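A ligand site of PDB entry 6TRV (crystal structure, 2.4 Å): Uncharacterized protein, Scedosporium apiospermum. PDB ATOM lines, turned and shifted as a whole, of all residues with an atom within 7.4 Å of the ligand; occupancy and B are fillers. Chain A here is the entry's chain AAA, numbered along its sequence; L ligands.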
ATOM      1  N   TYR A  71      16.979  36.057  -3.586  1.00  0.00           N
ATOM      2  CA  TYR A  71      17.626  34.773  -3.259  1.00  0.00           C
ATOM      3  C   TYR A  71      18.029  34.071  -4.558  1.00  0.00           C
ATOM      4  O   TYR A  71      17.202  33.806  -5.435  1.00  0.00           O
ATOM      5  CB  TYR A  71      16.705  33.871  -2.448  1.00  0.00           C
ATOM      6  CG  TYR A  71      16.289  34.411  -1.113  1.00  0.00           C
ATOM      7  CD1 TYR A  71      15.134  35.177  -0.956  1.00  0.00           C
ATOM      8  CD2 TYR A  71      17.032  34.134   0.023  1.00  0.00           C
ATOM      9  CE1 TYR A  71      14.765  35.672   0.290  1.00  0.00           C
ATOM     10  CE2 TYR A  71      16.693  34.635   1.269  1.00  0.00           C
ATOM     11  CZ  TYR A  71      15.556  35.407   1.406  1.00  0.00           C
ATOM     12  OH  TYR A  71      15.237  35.878   2.631  1.00  0.00           O
ATOM     13  N   ILE A  72      19.295  33.733  -4.685  1.00  0.00           N
ATOM     14  CA  ILE A  72      19.768  32.845  -5.756  1.00  0.00           C
ATOM     15  C   ILE A  72      20.389  31.655  -5.044  1.00  0.00           C
ATOM     16  O   ILE A  72      20.955  31.854  -3.996  1.00  0.00           O
ATOM     17  CB  ILE A  72      20.720  33.611  -6.671  1.00  0.00           C
ATOM     18  CG1 ILE A  72      20.081  34.901  -7.149  1.00  0.00           C
ATOM     19  CG2 ILE A  72      21.142  32.735  -7.837  1.00  0.00           C
ATOM     20  CD1 ILE A  72      21.029  35.838  -7.803  1.00  0.00           C
ATOM     21  N   ARG A  73      20.247  30.480  -5.640  1.00  0.00           N
ATOM     22  CA  ARG A  73      20.833  29.183  -5.245  1.00  0.00           C
ATOM     23  C   ARG A  73      21.378  28.513  -6.479  1.00  0.00           C
ATOM     24  O   ARG A  73      20.590  28.330  -7.402  1.00  0.00           O
ATOM     25  CB  ARG A  73      19.796  28.241  -4.616  1.00  0.00           C
ATOM     26  CG  ARG A  73      19.289  28.773  -3.289  1.00  0.00           C
ATOM     27  CD  ARG A  73      20.402  28.780  -2.274  1.00  0.00           C
ATOM     28  NE  ARG A  73      19.949  29.268  -0.980  1.00  0.00           N
ATOM     29  CZ  ARG A  73      19.838  30.556  -0.648  1.00  0.00           C
ATOM     30  NH1 ARG A  73      20.099  31.520  -1.516  1.00  0.00           N
ATOM     31  NH2 ARG A  73      19.495  30.879   0.598  1.00  0.00           N
ATOM     32  N   TYR A  75      23.528  25.104  -8.017  1.00  0.00           N
ATOM     33  CA  TYR A  75      23.874  23.718  -7.628  1.00  0.00           C
ATOM     34  C   TYR A  75      24.898  23.222  -8.643  1.00  0.00           C
ATOM     35  O   TYR A  75      24.766  23.501  -9.880  1.00  0.00           O
ATOM     36  CB  TYR A  75      22.638  22.816  -7.464  1.00  0.00           C
ATOM     37  CG  TYR A  75      21.688  23.364  -6.453  1.00  0.00           C
ATOM     38  CD1 TYR A  75      20.753  24.321  -6.786  1.00  0.00           C
ATOM     39  CD2 TYR A  75      21.793  23.029  -5.140  1.00  0.00           C
ATOM     40  CE1 TYR A  75      19.918  24.888  -5.839  1.00  0.00           C
ATOM     41  CE2 TYR A  75      20.980  23.576  -4.179  1.00  0.00           C
ATOM     42  CZ  TYR A  75      20.042  24.530  -4.526  1.00  0.00           C
ATOM     43  OH  TYR A  75      19.247  25.147  -3.576  1.00  0.00           O
ATOM     44  N   GLU A  85      26.048  23.646  -3.035  1.00  0.00           N
ATOM     45  CA  GLU A  85      25.126  24.787  -3.187  1.00  0.00           C
ATOM     46  C   GLU A  85      25.895  26.099  -2.914  1.00  0.00           C
ATOM     47  O   GLU A  85      26.551  26.251  -1.845  1.00  0.00           O
ATOM     48  CB  GLU A  85      23.903  24.537  -2.266  1.00  0.00           C
ATOM     49  CG  GLU A  85      22.890  25.654  -2.143  1.00  0.00           C
ATOM     50  CD  GLU A  85      21.917  25.438  -0.995  1.00  0.00           C
ATOM     51  OE1 GLU A  85      22.382  25.479   0.128  1.00  0.00           O
ATOM     52  OE2 GLU A  85      20.680  25.233  -1.252  1.00  0.00           O
ATOM     53  N   ALA A  86      25.848  27.034  -3.843  1.00  0.00           N
ATOM     54  CA  ALA A  86      26.349  28.409  -3.643  1.00  0.00           C
ATOM     55  C   ALA A  86      25.139  29.297  -3.359  1.00  0.00           C
ATOM     56  O   ALA A  86      24.100  29.053  -4.040  1.00  0.00           O
ATOM     57  CB  ALA A  86      27.144  28.861  -4.875  1.00  0.00           C
ATOM     58  N   CYS A  87      25.187  30.233  -2.408  1.00  0.00           N
ATOM     59  CA  CYS A  87      23.970  30.980  -1.977  1.00  0.00           C
ATOM     60  C   CYS A  87      24.184  32.481  -2.139  1.00  0.00           C
ATOM     61  O   CYS A  87      25.270  33.018  -1.770  1.00  0.00           O
ATOM     62  CB  CYS A  87      23.577  30.639  -0.558  1.00  0.00           C
ATOM     63  SG  CYS A  87      23.154  28.888  -0.323  1.00  0.00           S
ATOM     64  N   ASP A  89      21.988  35.874  -0.809  1.00  0.00           N
ATOM     65  CA  ASP A  89      20.904  36.436   0.000  1.00  0.00           C
ATOM     66  C   ASP A  89      21.094  37.958   0.081  1.00  0.00           C
ATOM     67  O   ASP A  89      20.823  38.528   1.144  1.00  0.00           O
ATOM     68  CB  ASP A  89      20.965  35.844   1.410  1.00  0.00           C
ATOM     69  CG  ASP A  89      20.664  34.337   1.578  1.00  0.00           C
ATOM     70  OD1 ASP A  89      20.494  33.602   0.575  1.00  0.00           O
ATOM     71  OD2 ASP A  89      20.602  33.918   2.736  1.00  0.00           O
ATOM     72  N   TYR A  94      27.763  32.660  -0.422  1.00  0.00           N
ATOM     73  CA  TYR A  94      28.255  31.836   0.693  1.00  0.00           C
ATOM     74  C   TYR A  94      27.864  30.397   0.388  1.00  0.00           C
ATOM     75  O   TYR A  94      26.957  30.202  -0.383  1.00  0.00           O
ATOM     76  CB  TYR A  94      27.713  32.403   2.027  1.00  0.00           C
ATOM     77  CG  TYR A  94      26.226  32.244   2.227  1.00  0.00           C
ATOM     78  CD1 TYR A  94      25.669  31.071   2.728  1.00  0.00           C
ATOM     79  CD2 TYR A  94      25.358  33.295   1.898  1.00  0.00           C
ATOM     80  CE1 TYR A  94      24.300  30.915   2.821  1.00  0.00           C
ATOM     81  CE2 TYR A  94      23.973  33.184   2.059  1.00  0.00           C
ATOM     82  CZ  TYR A  94      23.455  31.986   2.520  1.00  0.00           C
ATOM     83  OH  TYR A  94      22.097  31.905   2.676  1.00  0.00           O
ATOM     84  N   THR A  95      28.525  29.449   1.064  1.00  0.00           N
ATOM     85  CA  THR A  95      28.286  28.007   0.992  1.00  0.00           C
ATOM     86  C   THR A  95      27.001  27.680   1.750  1.00  0.00           C
ATOM     87  O   THR A  95      26.810  28.111   2.904  1.00  0.00           O
ATOM     88  CB  THR A  95      29.503  27.211   1.483  1.00  0.00           C
ATOM     89  OG1 THR A  95      30.575  27.495   0.610  1.00  0.00           O
ATOM     90  CG2 THR A  95      29.293  25.717   1.452  1.00  0.00           C
ATOM     91  N   GLY A  96      26.132  26.930   1.090  1.00  0.00           N
ATOM     92  CA  GLY A  96      24.841  26.550   1.676  1.00  0.00           C
ATOM     93  C   GLY A  96      24.932  25.196   2.363  1.00  0.00           C
ATOM     94  O   GLY A  96      25.941  24.499   2.149  1.00  0.00           O
ATOM     95  N   ALA A  97      23.890  24.821   3.086  1.00  0.00           N
ATOM     96  CA  ALA A  97      23.806  23.577   3.862  1.00  0.00           C
ATOM     97  C   ALA A  97      23.544  22.377   2.936  1.00  0.00           C
ATOM     98  O   ALA A  97      23.665  21.243   3.352  1.00  0.00           O
ATOM     99  CB  ALA A  97      22.724  23.790   4.903  1.00  0.00           C
ATOM    100  N   PHE A  98      23.156  22.594   1.708  1.00  0.00           N
ATOM    101  CA  PHE A  98      22.845  21.475   0.790  1.00  0.00           C
ATOM    102  C   PHE A  98      24.135  20.711   0.442  1.00  0.00           C
ATOM    103  O   PHE A  98      25.012  21.273  -0.158  1.00  0.00           O
ATOM    104  CB  PHE A  98      22.113  22.000  -0.456  1.00  0.00           C
ATOM    105  CG  PHE A  98      21.758  20.895  -1.411  1.00  0.00           C
ATOM    106  CD1 PHE A  98      20.654  20.090  -1.193  1.00  0.00           C
ATOM    107  CD2 PHE A  98      22.656  20.530  -2.405  1.00  0.00           C
ATOM    108  CE1 PHE A  98      20.400  19.007  -2.004  1.00  0.00           C
ATOM    109  CE2 PHE A  98      22.385  19.463  -3.238  1.00  0.00           C
ATOM    110  CZ  PHE A  98      21.257  18.702  -3.038  1.00  0.00           C
ATOM    111  N   VAL A  99      24.229  19.443   0.839  1.00  0.00           N
ATOM    112  CA  VAL A  99      25.329  18.494   0.502  1.00  0.00           C
ATOM    113  C   VAL A  99      24.716  17.100   0.301  1.00  0.00           C
ATOM    114  O   VAL A  99      24.149  16.568   1.265  1.00  0.00           O
ATOM    115  CB  VAL A  99      26.477  18.419   1.556  1.00  0.00           C
ATOM    116  CG1 VAL A  99      27.626  17.535   1.026  1.00  0.00           C
ATOM    117  CG2 VAL A  99      26.989  19.810   1.971  1.00  0.00           C
ATOM    118  N   PHE A 112      12.807  27.077  -6.916  1.00  0.00           N
ATOM    119  CA  PHE A 112      12.151  27.731  -5.782  1.00  0.00           C
ATOM    120  C   PHE A 112      10.674  27.446  -5.912  1.00  0.00           C
ATOM    121  O   PHE A 112      10.222  27.362  -6.956  1.00  0.00           O
ATOM    122  CB  PHE A 112      12.526  29.206  -5.730  1.00  0.00           C
ATOM    123  CG  PHE A 112      13.726  29.453  -4.855  1.00  0.00           C
ATOM    124  CD1 PHE A 112      13.648  29.233  -3.491  1.00  0.00           C
ATOM    125  CD2 PHE A 112      14.905  29.911  -5.374  1.00  0.00           C
ATOM    126  CE1 PHE A 112      14.737  29.457  -2.669  1.00  0.00           C
ATOM    127  CE2 PHE A 112      15.982  30.169  -4.541  1.00  0.00           C
ATOM    128  CZ  PHE A 112      15.900  29.919  -3.199  1.00  0.00           C
ATOM    129  N   ILE A 117      10.847  31.036   0.711  1.00  0.00           N
ATOM    130  CA  ILE A 117      12.166  30.403   0.522  1.00  0.00           C
ATOM    131  C   ILE A 117      11.889  28.926   0.752  1.00  0.00           C
ATOM    132  O   ILE A 117      11.963  28.540   1.889  1.00  0.00           O
ATOM    133  CB  ILE A 117      13.164  31.047   1.499  1.00  0.00           C
ATOM    134  CG1 ILE A 117      12.928  32.561   1.555  1.00  0.00           C
ATOM    135  CG2 ILE A 117      14.591  30.659   1.180  1.00  0.00           C
ATOM    136  CD1 ILE A 117      12.583  33.155   0.227  1.00  0.00           C
ATOM    137  N   VAL A 118      11.531  28.191  -0.299  1.00  0.00           N
ATOM    138  CA  VAL A 118      11.209  26.740  -0.293  1.00  0.00           C
ATOM    139  C   VAL A 118      11.872  26.113  -1.552  1.00  0.00           C
ATOM    140  O   VAL A 118      11.694  26.622  -2.648  1.00  0.00           O
ATOM    141  CB  VAL A 118       9.676  26.555  -0.255  1.00  0.00           C
ATOM    142  CG1 VAL A 118       9.329  25.088  -0.417  1.00  0.00           C
ATOM    143  CG2 VAL A 118       8.987  27.129   0.984  1.00  0.00           C
ATOM    144  N   VAL A 119      12.661  25.070  -1.414  1.00  0.00           N
ATOM    145  CA  VAL A 119      13.535  24.642  -2.530  1.00  0.00           C
ATOM    146  C   VAL A 119      13.353  23.140  -2.756  1.00  0.00           C
ATOM    147  O   VAL A 119      13.153  22.395  -1.813  1.00  0.00           O
ATOM    148  CB  VAL A 119      15.012  24.978  -2.284  1.00  0.00           C
ATOM    149  CG1 VAL A 119      15.824  25.011  -3.582  1.00  0.00           C
ATOM    150  CG2 VAL A 119      15.180  26.281  -1.543  1.00  0.00           C
ATOM    151  N   VAL A 121      15.434  20.138  -5.061  1.00  0.00           N
ATOM    152  CA  VAL A 121      16.601  19.765  -5.882  1.00  0.00           C
ATOM    153  C   VAL A 121      16.415  18.306  -6.279  1.00  0.00           C
ATOM    154  O   VAL A 121      16.039  17.489  -5.394  1.00  0.00           O
ATOM    155  CB  VAL A 121      17.862  19.983  -5.059  1.00  0.00           C
ATOM    156  CG1 VAL A 121      19.085  19.877  -5.922  1.00  0.00           C
ATOM    157  CG2 VAL A 121      17.813  21.312  -4.306  1.00  0.00           C
ATOM    158  N   TRP A 135      13.731  21.372   1.069  1.00  0.00           N
ATOM    159  CA  TRP A 135      13.968  22.396   2.117  1.00  0.00           C
ATOM    160  C   TRP A 135      12.711  23.221   2.306  1.00  0.00           C
ATOM    161  O   TRP A 135      12.364  23.922   1.340  1.00  0.00           O
ATOM    162  CB  TRP A 135      15.146  23.267   1.789  1.00  0.00           C
ATOM    163  CG  TRP A 135      15.249  24.425   2.742  1.00  0.00           C
ATOM    164  CD1 TRP A 135      14.471  25.548   2.829  1.00  0.00           C
ATOM    165  CD2 TRP A 135      16.225  24.519   3.776  1.00  0.00           C
ATOM    166  NE1 TRP A 135      14.881  26.368   3.866  1.00  0.00           N
ATOM    167  CE2 TRP A 135      15.963  25.745   4.454  1.00  0.00           C
ATOM    168  CE3 TRP A 135      17.249  23.654   4.182  1.00  0.00           C
ATOM    169  CZ2 TRP A 135      16.769  26.182   5.485  1.00  0.00           C
ATOM    170  CZ3 TRP A 135      18.042  24.071   5.205  1.00  0.00           C
ATOM    171  CH2 TRP A 135      17.796  25.314   5.854  1.00  0.00           C
ATOM    172  N   SER A 137      12.009  24.781   5.640  1.00  0.00           N
ATOM    173  CA  SER A 137      12.436  25.811   6.610  1.00  0.00           C
ATOM    174  C   SER A 137      13.717  25.370   7.304  1.00  0.00           C
ATOM    175  O   SER A 137      14.073  24.183   7.246  1.00  0.00           O
ATOM    176  CB  SER A 137      11.352  26.077   7.626  1.00  0.00           C
ATOM    177  OG  SER A 137      11.321  25.006   8.547  1.00  0.00           O
ATOM    178  N   PRO A 138      14.380  26.303   8.037  1.00  0.00           N
ATOM    179  CA  PRO A 138      15.625  26.005   8.732  1.00  0.00           C
ATOM    180  C   PRO A 138      15.456  25.003   9.875  1.00  0.00           C
ATOM    181  O   PRO A 138      16.375  24.294  10.161  1.00  0.00           O
ATOM    182  CB  PRO A 138      16.047  27.345   9.345  1.00  0.00           C
ATOM    183  CG  PRO A 138      15.225  28.382   8.574  1.00  0.00           C
ATOM    184  CD  PRO A 138      13.938  27.692   8.256  1.00  0.00           C
ATOM    185  N   GLY A 141      15.355  21.682   7.971  1.00  0.00           N
ATOM    186  CA  GLY A 141      16.423  21.575   6.970  1.00  0.00           C
ATOM    187  C   GLY A 141      16.137  20.611   5.795  1.00  0.00           C
ATOM    188  O   GLY A 141      14.944  20.321   5.503  1.00  0.00           O
ATOM    189  N   TRP A 142      17.201  20.157   5.131  1.00  0.00           N
ATOM    190  CA  TRP A 142      17.121  19.250   3.989  1.00  0.00           C
ATOM    191  C   TRP A 142      16.566  17.904   4.407  1.00  0.00           C
ATOM    192  O   TRP A 142      17.172  17.306   5.202  1.00  0.00           O
ATOM    193  CB  TRP A 142      18.463  19.181   3.270  1.00  0.00           C
ATOM    194  CG  TRP A 142      18.772  20.492   2.587  1.00  0.00           C
ATOM    195  CD1 TRP A 142      19.539  21.503   3.084  1.00  0.00           C
ATOM    196  CD2 TRP A 142      18.218  20.982   1.339  1.00  0.00           C
ATOM    197  NE1 TRP A 142      19.553  22.544   2.186  1.00  0.00           N
ATOM    198  CE2 TRP A 142      18.804  22.232   1.089  1.00  0.00           C
ATOM    199  CE3 TRP A 142      17.350  20.448   0.378  1.00  0.00           C
ATOM    200  CZ2 TRP A 142      18.489  22.982  -0.041  1.00  0.00           C
ATOM    201  CZ3 TRP A 142      17.098  21.165  -0.773  1.00  0.00           C
ATOM    202  CH2 TRP A 142      17.632  22.432  -0.957  1.00  0.00           C
HETATM  203  C1  LIG L   1      20.218  28.628   3.210  1.00  0.00           C
HETATM  204  C2  LIG L   1      21.013  27.425   2.723  1.00  0.00           C
HETATM  205  C3  LIG L   1      20.067  26.235   2.610  1.00  0.00           C
HETATM  206  C4  LIG L   1      18.859  26.547   1.765  1.00  0.00           C
HETATM  207  C5  LIG L   1      18.185  27.808   2.354  1.00  0.00           C
HETATM  208  C6  LIG L   1      16.972  28.279   1.544  1.00  0.00           C
HETATM  209  O1  LIG L   1      19.721  28.309   4.506  1.00  0.00           O
HETATM  210  O2  LIG L   1      22.070  27.149   3.697  1.00  0.00           O
HETATM  211  O3  LIG L   1      20.815  25.014   2.204  1.00  0.00           O
HETATM  212  O4  LIG L   1      19.274  26.747   0.362  1.00  0.00           O
HETATM  213  O5  LIG L   1      19.164  28.821   2.282  1.00  0.00           O
HETATM  214  C7  LIG L   1      19.237  29.444   5.206  1.00  0.00           C
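OE2 of Glu 85 lies within hydrogen-bond range of O4 of the ligand, at 2.6 Å. NH2 of Arg 73 is in hydrogen-bond range of O5 of the ligand (2.7 Å). NE1 of Trp 142 lies within hydrogen-bond range of O3 of the ligand, at 2.8 Å. An oxygen (O2) of the ligand is in hydrogen-bond range of the backbone NH (N) of Ala 97 (3.0 Å). An oxygen (O3) of the ligand lies within hydrogen-bond range of the backbone NH (N) of Phe 98 (3.4 Å).
OE1 of Glu 85 is in hydrogen-bond range of N of Ala 97 (3.4 Å). N of Phe 98 is in hydrogen-bond range of OE1 of Glu 85 (3.4 Å). The backbone carbonyl oxygen (O) of Glu 85 sits at hydrogen-bond distance from the backbone NH (N) of Gly 96. The side-chain carboxylate (OE1) of Glu 85 is in hydrogen-bond range of the side-chain sulfur (SG) of Cys 87, at 3.5 Å. OE2 of Glu 85 lies within hydrogen-bond range of OH of Tyr 75 (2.7 Å). The guanidinium group (NE) of Arg 73 is in hydrogen-bond range of the side-chain sulfur (SG) of Cys 87 (3.3 Å). The backbone NH of Val 119 lies within hydrogen-bond range of the backbone carbonyl oxygen of Trp 135 (3.0 Å). O of Tyr 94 is in hydrogen-bond range of N of Cys 87, at 2.7 Å.
Tyr 94 touches the ligand. Gly 96 touches the ligand. CG2 of Ile 117 touches C6 of the ligand, at 3.4 Å. Trp 135 touches the ligand (NE1 to C6, 3.7 Å). Of the 24 residues printed, 9 come within 4 Å of the ligand. Along chain A the residues within 4 Å of the ligand span positions 73 to 142.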
